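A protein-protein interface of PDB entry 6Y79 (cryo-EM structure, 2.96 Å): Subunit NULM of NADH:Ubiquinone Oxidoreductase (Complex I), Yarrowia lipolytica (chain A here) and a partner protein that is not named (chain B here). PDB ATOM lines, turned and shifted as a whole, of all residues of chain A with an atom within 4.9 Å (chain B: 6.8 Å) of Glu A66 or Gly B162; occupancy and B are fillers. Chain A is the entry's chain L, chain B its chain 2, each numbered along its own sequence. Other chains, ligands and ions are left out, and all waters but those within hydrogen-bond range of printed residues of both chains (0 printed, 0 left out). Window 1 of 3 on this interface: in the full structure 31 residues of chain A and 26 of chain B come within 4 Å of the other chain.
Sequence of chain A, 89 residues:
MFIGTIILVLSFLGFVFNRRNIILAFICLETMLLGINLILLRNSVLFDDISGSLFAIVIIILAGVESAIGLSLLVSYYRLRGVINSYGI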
ATOM      1  N   LEU A  29       7.722 -18.937 -15.417  1.00  0.00           N
ATOM      2  CA  LEU A  29       9.184 -18.911 -15.500  1.00  0.00           C
ATOM      3  C   LEU A  29       9.832 -19.090 -14.126  1.00  0.00           C
ATOM      4  O   LEU A  29      10.778 -19.880 -13.958  1.00  0.00           O
ATOM      5  CB  LEU A  29       9.619 -17.592 -16.138  1.00  0.00           C
ATOM      6  CG  LEU A  29      11.043 -17.358 -16.631  1.00  0.00           C
ATOM      7  CD1 LEU A  29      11.013 -16.566 -17.921  1.00  0.00           C
ATOM      8  CD2 LEU A  29      11.859 -16.617 -15.587  1.00  0.00           C
ATOM      9  N   LEU A  62      20.624 -15.297  -9.510  1.00  0.00           N
ATOM     10  CA  LEU A  62      20.387 -15.038 -10.927  1.00  0.00           C
ATOM     11  C   LEU A  62      18.898 -14.995 -11.262  1.00  0.00           C
ATOM     12  O   LEU A  62      18.484 -14.186 -12.099  1.00  0.00           O
ATOM     13  CB  LEU A  62      21.112 -16.083 -11.769  1.00  0.00           C
ATOM     14  CG  LEU A  62      22.632 -15.938 -11.695  1.00  0.00           C
ATOM     15  CD1 LEU A  62      23.327 -17.035 -12.432  1.00  0.00           C
ATOM     16  CD2 LEU A  62      23.056 -14.630 -12.261  1.00  0.00           C
ATOM     17  N   ALA A  63      18.079 -15.814 -10.593  1.00  0.00           N
ATOM     18  CA  ALA A  63      16.631 -15.743 -10.773  1.00  0.00           C
ATOM     19  C   ALA A  63      16.069 -14.420 -10.273  1.00  0.00           C
ATOM     20  O   ALA A  63      15.193 -13.826 -10.919  1.00  0.00           O
ATOM     21  CB  ALA A  63      15.958 -16.904 -10.048  1.00  0.00           C
ATOM     22  N   GLY A  64      16.573 -13.942  -9.133  1.00  0.00           N
ATOM     23  CA  GLY A  64      16.153 -12.639  -8.637  1.00  0.00           C
ATOM     24  C   GLY A  64      16.496 -11.503  -9.584  1.00  0.00           C
ATOM     25  O   GLY A  64      15.643 -10.665  -9.903  1.00  0.00           O
ATOM     26  N   VAL A  65      17.738 -11.486 -10.080  1.00  0.00           N
ATOM     27  CA  VAL A  65      18.173 -10.435 -10.999  1.00  0.00           C
ATOM     28  C   VAL A  65      17.400 -10.495 -12.312  1.00  0.00           C
ATOM     29  O   VAL A  65      17.041  -9.450 -12.863  1.00  0.00           O
ATOM     30  CB  VAL A  65      19.699 -10.512 -11.217  1.00  0.00           C
ATOM     31  CG1 VAL A  65      20.176  -9.509 -12.259  1.00  0.00           C
ATOM     32  CG2 VAL A  65      20.416 -10.230  -9.927  1.00  0.00           C
ATOM     33  N   GLU A  66      17.059 -11.696 -12.796  1.00  0.00           N
ATOM     34  CA  GLU A  66      16.276 -11.781 -14.027  1.00  0.00           C
ATOM     35  C   GLU A  66      14.856 -11.272 -13.816  1.00  0.00           C
ATOM     36  O   GLU A  66      14.290 -10.624 -14.705  1.00  0.00           O
ATOM     37  CB  GLU A  66      16.251 -13.209 -14.578  1.00  0.00           C
ATOM     38  CG  GLU A  66      15.637 -13.222 -15.973  1.00  0.00           C
ATOM     39  CD  GLU A  66      15.636 -14.546 -16.703  1.00  0.00           C
ATOM     40  OE1 GLU A  66      16.188 -15.534 -16.186  1.00  0.00           O
ATOM     41  OE2 GLU A  66      15.049 -14.592 -17.805  1.00  0.00           O
ATOM     42  N   SER A  67      14.283 -11.509 -12.631  1.00  0.00           N
ATOM     43  CA  SER A  67      12.966 -10.954 -12.320  1.00  0.00           C
ATOM     44  C   SER A  67      12.986  -9.431 -12.287  1.00  0.00           C
ATOM     45  O   SER A  67      12.089  -8.780 -12.829  1.00  0.00           O
ATOM     46  CB  SER A  67      12.466 -11.508 -10.993  1.00  0.00           C
ATOM     47  OG  SER A  67      12.398 -12.916 -11.040  1.00  0.00           O
ATOM     48  N   ALA A  68      14.028  -8.848 -11.692  1.00  0.00           N
ATOM     49  CA  ALA A  68      14.147  -7.389 -11.650  1.00  0.00           C
ATOM     50  C   ALA A  68      14.304  -6.796 -13.049  1.00  0.00           C
ATOM     51  O   ALA A  68      13.593  -5.842 -13.415  1.00  0.00           O
ATOM     52  CB  ALA A  68      15.325  -6.996 -10.763  1.00  0.00           C
ATOM     53  N   ILE A  69      15.209  -7.380 -13.851  1.00  0.00           N
ATOM     54  CA  ILE A  69      15.464  -6.932 -15.224  1.00  0.00           C
ATOM     55  C   ILE A  69      14.196  -7.016 -16.061  1.00  0.00           C
ATOM     56  O   ILE A  69      13.768  -6.035 -16.676  1.00  0.00           O
ATOM     57  CB  ILE A  69      16.594  -7.760 -15.867  1.00  0.00           C
ATOM     58  CG1 ILE A  69      17.954  -7.483 -15.232  1.00  0.00           C
ATOM     59  CG2 ILE A  69      16.679  -7.490 -17.356  1.00  0.00           C
ATOM     60  CD1 ILE A  69      18.418  -6.092 -15.348  1.00  0.00           C
ATOM     61  N   GLY A  70      13.559  -8.187 -16.071  1.00  0.00           N
ATOM     62  CA  GLY A  70      12.398  -8.405 -16.907  1.00  0.00           C
ATOM     63  C   GLY A  70      11.168  -7.645 -16.487  1.00  0.00           C
ATOM     64  O   GLY A  70      10.345  -7.300 -17.340  1.00  0.00           O
ATOM     65  N   LEU A  71      11.034  -7.327 -15.205  1.00  0.00           N
ATOM     66  CA  LEU A  71       9.870  -6.545 -14.830  1.00  0.00           C
ATOM     67  C   LEU A  71      10.075  -5.072 -15.147  1.00  0.00           C
ATOM     68  O   LEU A  71       9.108  -4.385 -15.498  1.00  0.00           O
ATOM     69  CB  LEU A  71       9.529  -6.773 -13.358  1.00  0.00           C
ATOM     70  CG  LEU A  71       8.511  -7.895 -13.089  1.00  0.00           C
ATOM     71  CD1 LEU A  71       7.207  -7.623 -13.779  1.00  0.00           C
ATOM     72  CD2 LEU A  71       8.977  -9.245 -13.543  1.00  0.00           C
ATOM     73  N   GLU B 131      23.995 -15.813 -18.443  1.00  0.00           N
ATOM     74  CA  GLU B 131      22.941 -14.919 -17.981  1.00  0.00           C
ATOM     75  C   GLU B 131      23.401 -13.473 -17.938  1.00  0.00           C
ATOM     76  O   GLU B 131      22.596 -12.569 -18.165  1.00  0.00           O
ATOM     77  CB  GLU B 131      22.391 -15.367 -16.633  1.00  0.00           C
ATOM     78  CG  GLU B 131      21.143 -16.136 -16.874  1.00  0.00           C
ATOM     79  CD  GLU B 131      21.450 -17.458 -17.523  1.00  0.00           C
ATOM     80  OE1 GLU B 131      22.211 -18.222 -16.917  1.00  0.00           O
ATOM     81  OE2 GLU B 131      21.041 -17.620 -18.681  1.00  0.00           O
ATOM     82  N   TYR B 135      21.068 -10.937 -20.018  1.00  0.00           N
ATOM     83  CA  TYR B 135      20.469  -9.724 -19.469  1.00  0.00           C
ATOM     84  C   TYR B 135      20.991  -8.493 -20.181  1.00  0.00           C
ATOM     85  O   TYR B 135      20.250  -7.521 -20.376  1.00  0.00           O
ATOM     86  CB  TYR B 135      20.742  -9.570 -17.976  1.00  0.00           C
ATOM     87  CG  TYR B 135      20.476 -10.738 -17.062  1.00  0.00           C
ATOM     88  CD1 TYR B 135      19.528 -11.702 -17.359  1.00  0.00           C
ATOM     89  CD2 TYR B 135      21.188 -10.860 -15.879  1.00  0.00           C
ATOM     90  CE1 TYR B 135      19.312 -12.759 -16.514  1.00  0.00           C
ATOM     91  CE2 TYR B 135      20.978 -11.908 -15.032  1.00  0.00           C
ATOM     92  CZ  TYR B 135      20.039 -12.852 -15.351  1.00  0.00           C
ATOM     93  OH  TYR B 135      19.827 -13.899 -14.501  1.00  0.00           O
ATOM     94  N   TYR B 138      18.980  -8.256 -23.392  1.00  0.00           N
ATOM     95  CA  TYR B 138      17.659  -7.733 -23.006  1.00  0.00           C
ATOM     96  C   TYR B 138      17.677  -6.214 -22.880  1.00  0.00           C
ATOM     97  O   TYR B 138      16.827  -5.512 -23.441  1.00  0.00           O
ATOM     98  CB  TYR B 138      17.192  -8.294 -21.658  1.00  0.00           C
ATOM     99  CG  TYR B 138      17.074  -9.786 -21.459  1.00  0.00           C
ATOM    100  CD1 TYR B 138      16.989 -10.641 -22.511  1.00  0.00           C
ATOM    101  CD2 TYR B 138      17.015 -10.321 -20.185  1.00  0.00           C
ATOM    102  CE1 TYR B 138      16.894 -11.998 -22.336  1.00  0.00           C
ATOM    103  CE2 TYR B 138      16.915 -11.673 -19.985  1.00  0.00           C
ATOM    104  CZ  TYR B 138      16.845 -12.506 -21.069  1.00  0.00           C
ATOM    105  OH  TYR B 138      16.737 -13.858 -20.879  1.00  0.00           O
ATOM    106  N   LEU B 156       9.793 -10.169 -26.170  1.00  0.00           N
ATOM    107  CA  LEU B 156       9.887 -11.472 -26.823  1.00  0.00           C
ATOM    108  C   LEU B 156      11.230 -12.133 -26.557  1.00  0.00           C
ATOM    109  O   LEU B 156      11.297 -13.338 -26.276  1.00  0.00           O
ATOM    110  CB  LEU B 156       9.667 -11.297 -28.324  1.00  0.00           C
ATOM    111  CG  LEU B 156       9.365 -12.485 -29.226  1.00  0.00           C
ATOM    112  CD1 LEU B 156       8.487 -12.002 -30.312  1.00  0.00           C
ATOM    113  CD2 LEU B 156      10.595 -12.977 -29.851  1.00  0.00           C
ATOM    114  N   TYR B 157      12.306 -11.352 -26.620  1.00  0.00           N
ATOM    115  CA  TYR B 157      13.631 -11.892 -26.388  1.00  0.00           C
ATOM    116  C   TYR B 157      13.821 -12.293 -24.939  1.00  0.00           C
ATOM    117  O   TYR B 157      14.507 -13.283 -24.676  1.00  0.00           O
ATOM    118  CB  TYR B 157      14.694 -10.884 -26.815  1.00  0.00           C
ATOM    119  CG  TYR B 157      16.075 -11.465 -26.770  1.00  0.00           C
ATOM    120  CD1 TYR B 157      16.527 -12.369 -27.712  1.00  0.00           C
ATOM    121  CD2 TYR B 157      16.911 -11.126 -25.767  1.00  0.00           C
ATOM    122  CE1 TYR B 157      17.793 -12.902 -27.635  1.00  0.00           C
ATOM    123  CE2 TYR B 157      18.151 -11.671 -25.645  1.00  0.00           C
ATOM    124  CZ  TYR B 157      18.605 -12.537 -26.597  1.00  0.00           C
ATOM    125  OH  TYR B 157      19.875 -13.046 -26.476  1.00  0.00           O
ATOM    126  N   PHE B 158      13.188 -11.577 -24.001  1.00  0.00           N
ATOM    127  CA  PHE B 158      13.221 -11.971 -22.596  1.00  0.00           C
ATOM    128  C   PHE B 158      12.619 -13.350 -22.382  1.00  0.00           C
ATOM    129  O   PHE B 158      13.232 -14.209 -21.741  1.00  0.00           O
ATOM    130  CB  PHE B 158      12.476 -10.953 -21.743  1.00  0.00           C
ATOM    131  CG  PHE B 158      12.426 -11.321 -20.295  1.00  0.00           C
ATOM    132  CD1 PHE B 158      13.536 -11.148 -19.509  1.00  0.00           C
ATOM    133  CD2 PHE B 158      11.279 -11.850 -19.719  1.00  0.00           C
ATOM    134  CE1 PHE B 158      13.520 -11.494 -18.197  1.00  0.00           C
ATOM    135  CE2 PHE B 158      11.266 -12.200 -18.393  1.00  0.00           C
ATOM    136  CZ  PHE B 158      12.388 -12.017 -17.632  1.00  0.00           C
ATOM    137  N   PHE B 159      11.419 -13.583 -22.916  1.00  0.00           N
ATOM    138  CA  PHE B 159      10.763 -14.865 -22.647  1.00  0.00           C
ATOM    139  C   PHE B 159      11.440 -16.021 -23.377  1.00  0.00           C
ATOM    140  O   PHE B 159      11.639 -17.107 -22.798  1.00  0.00           O
ATOM    141  CB  PHE B 159       9.293 -14.788 -23.012  1.00  0.00           C
ATOM    142  CG  PHE B 159       8.495 -13.955 -22.071  1.00  0.00           C
ATOM    143  CD1 PHE B 159       8.269 -14.378 -20.777  1.00  0.00           C
ATOM    144  CD2 PHE B 159       7.978 -12.745 -22.475  1.00  0.00           C
ATOM    145  CE1 PHE B 159       7.549 -13.607 -19.914  1.00  0.00           C
ATOM    146  CE2 PHE B 159       7.260 -11.971 -21.613  1.00  0.00           C
ATOM    147  CZ  PHE B 159       7.043 -12.406 -20.338  1.00  0.00           C
ATOM    148  N   MET B 160      11.840 -15.803 -24.632  1.00  0.00           N
ATOM    149  CA  MET B 160      12.496 -16.876 -25.364  1.00  0.00           C
ATOM    150  C   MET B 160      13.928 -17.115 -24.910  1.00  0.00           C
ATOM    151  O   MET B 160      14.452 -18.204 -25.144  1.00  0.00           O
ATOM    152  CB  MET B 160      12.471 -16.582 -26.852  1.00  0.00           C
ATOM    153  CG  MET B 160      11.099 -16.385 -27.433  1.00  0.00           C
ATOM    154  SD  MET B 160      10.170 -17.901 -27.595  1.00  0.00           S
ATOM    155  CE  MET B 160       8.946 -17.679 -26.312  1.00  0.00           C
ATOM    156  N   GLY B 161      14.579 -16.146 -24.265  1.00  0.00           N
ATOM    157  CA  GLY B 161      15.854 -16.429 -23.640  1.00  0.00           C
ATOM    158  C   GLY B 161      15.711 -17.070 -22.281  1.00  0.00           C
ATOM    159  O   GLY B 161      16.570 -17.860 -21.877  1.00  0.00           O
ATOM    160  N   GLY B 162      14.617 -16.769 -21.575  1.00  0.00           N
ATOM    161  CA  GLY B 162      14.380 -17.395 -20.287  1.00  0.00           C
ATOM    162  C   GLY B 162      14.146 -18.887 -20.387  1.00  0.00           C
ATOM    163  O   GLY B 162      14.698 -19.654 -19.589  1.00  0.00           O
ATOM    164  N   ILE B 163      13.348 -19.319 -21.377  1.00  0.00           N
ATOM    165  CA  ILE B 163      13.119 -20.757 -21.580  1.00  0.00           C
ATOM    166  C   ILE B 163      14.424 -21.481 -21.882  1.00  0.00           C
ATOM    167  O   ILE B 163      14.735 -22.523 -21.294  1.00  0.00           O
ATOM    168  CB  ILE B 163      12.123 -21.009 -22.721  1.00  0.00           C
ATOM    169  CG1 ILE B 163      10.803 -20.317 -22.511  1.00  0.00           C
ATOM    170  CG2 ILE B 163      11.872 -22.497 -22.886  1.00  0.00           C
ATOM    171  CD1 ILE B 163      10.024 -20.348 -23.797  1.00  0.00           C
ATOM    172  N   LEU B 164      15.203 -20.941 -22.803  1.00  0.00           N
ATOM    173  CA  LEU B 164      16.398 -21.621 -23.258  1.00  0.00           C
ATOM    174  C   LEU B 164      17.564 -21.455 -22.307  1.00  0.00           C
ATOM    175  O   LEU B 164      18.612 -22.059 -22.538  1.00  0.00           O
ATOM    176  CB  LEU B 164      16.765 -21.123 -24.649  1.00  0.00           C
ATOM    177  CG  LEU B 164      15.599 -21.454 -25.565  1.00  0.00           C
ATOM    178  CD1 LEU B 164      15.722 -20.721 -26.864  1.00  0.00           C
ATOM    179  CD2 LEU B 164      15.512 -22.953 -25.780  1.00  0.00           C
ATOM    180  N   SER B 165      17.413 -20.626 -21.275  1.00  0.00           N
ATOM    181  CA  SER B 165      18.345 -20.637 -20.158  1.00  0.00           C
ATOM    182  C   SER B 165      17.968 -21.657 -19.102  1.00  0.00           C
ATOM    183  O   SER B 165      18.848 -22.295 -18.511  1.00  0.00           O
ATOM    184  CB  SER B 165      18.402 -19.256 -19.547  1.00  0.00           C
ATOM    185  OG  SER B 165      19.140 -18.406 -20.410  1.00  0.00           O
ATOM    186  N   ILE B 166      16.668 -21.837 -18.870  1.00  0.00           N
ATOM    187  CA  ILE B 166      16.229 -22.898 -17.977  1.00  0.00           C
ATOM    188  C   ILE B 166      16.508 -24.277 -18.572  1.00  0.00           C
ATOM    189  O   ILE B 166      16.797 -25.219 -17.828  1.00  0.00           O
ATOM    190  CB  ILE B 166      14.750 -22.653 -17.626  1.00  0.00           C
ATOM    191  CG1 ILE B 166      14.638 -21.355 -16.834  1.00  0.00           C
ATOM    192  CG2 ILE B 166      14.163 -23.752 -16.776  1.00  0.00           C
ATOM    193  CD1 ILE B 166      13.242 -20.889 -16.628  1.00  0.00           C
ATOM    194  N   LEU B 167      16.517 -24.403 -19.899  1.00  0.00           N
ATOM    195  CA  LEU B 167      16.901 -25.672 -20.518  1.00  0.00           C
ATOM    196  C   LEU B 167      18.389 -25.974 -20.325  1.00  0.00           C
ATOM    197  O   LEU B 167      18.767 -27.130 -20.088  1.00  0.00           O
ATOM    198  CB  LEU B 167      16.535 -25.656 -22.002  1.00  0.00           C
ATOM    199  CG  LEU B 167      16.824 -26.905 -22.833  1.00  0.00           C
ATOM    200  CD1 LEU B 167      16.139 -28.119 -22.248  1.00  0.00           C
ATOM    201  CD2 LEU B 167      16.393 -26.697 -24.263  1.00  0.00           C
ATOM    202  N   LYS B 211      19.589 -20.389 -28.946  1.00  0.00           N
ATOM    203  CA  LYS B 211      19.813 -18.960 -28.778  1.00  0.00           C
ATOM    204  C   LYS B 211      20.534 -18.332 -29.959  1.00  0.00           C
ATOM    205  O   LYS B 211      20.455 -17.116 -30.134  1.00  0.00           O
ATOM    206  CB  LYS B 211      20.623 -18.718 -27.517  1.00  0.00           C
ATOM    207  CG  LYS B 211      19.961 -19.243 -26.283  1.00  0.00           C
ATOM    208  CD  LYS B 211      20.717 -18.840 -25.056  1.00  0.00           C
ATOM    209  CE  LYS B 211      19.816 -18.919 -23.865  1.00  0.00           C
ATOM    210  NZ  LYS B 211      20.487 -18.422 -22.653  1.00  0.00           N
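The backbone carbonyl oxygen (O) of Leu A62 is in hydrogen-bond range of the side-chain hydroxyl (OH) of Tyr B135, 2.8 Å away.
Among the printed residues, merely in contact across the chains: Glu A66 with Phe B158, Gly A70 with Phe B158, Glu A66 with Tyr B138, Glu A66 with Tyr B135, Val A65 with Tyr B135, Leu A29 with Ile B166 and Glu A66 with Gly B162.
Of the printed residues of chain B, Leu A29 touches Ile B166 (3.8 Å).
Printed residues of chain B within 4 Å of Val A65: Tyr B135.
Of the printed residues of chain B, Glu A66 touches Tyr B135 (3.6 Å), Tyr B138 (3.6 Å), Phe B158 (3.5 Å) and Gly B162 (3.8 Å).
Ser A67 touches none of the printed residues of chain B.
Leu A71 touches none of the printed residues of chain B.
Printed residues of chain A within 4 Å of Tyr B135: Leu A62, Val A65 and Glu A66.
Of the printed residues of chain A, Phe B158 touches Glu A66 (3.5 Å) and Gly A70 (3.5 Å).
The nearest printed residue of chain B that does not touch Leu A62 is Glu B131 (4.5 Å).
Printed residues of chain B that touch a printed residue of chain A: Tyr B135, Tyr B138, Phe B158, Gly B162 and Ile B166.
Hydrophobic or aromatic side chains of chain B within 4 Å of the printed part of chain A: Tyr B135, Tyr B138, Phe B158 and Ile B166.
Hydrophobic or aromatic side chains of chain A that line the printed part of chain B: Leu A62 and Val A65.
Among the printed residues, no Asp or Glu carboxylate lies within 4 Å of a Lys or Arg side-chain nitrogen of the other chain.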
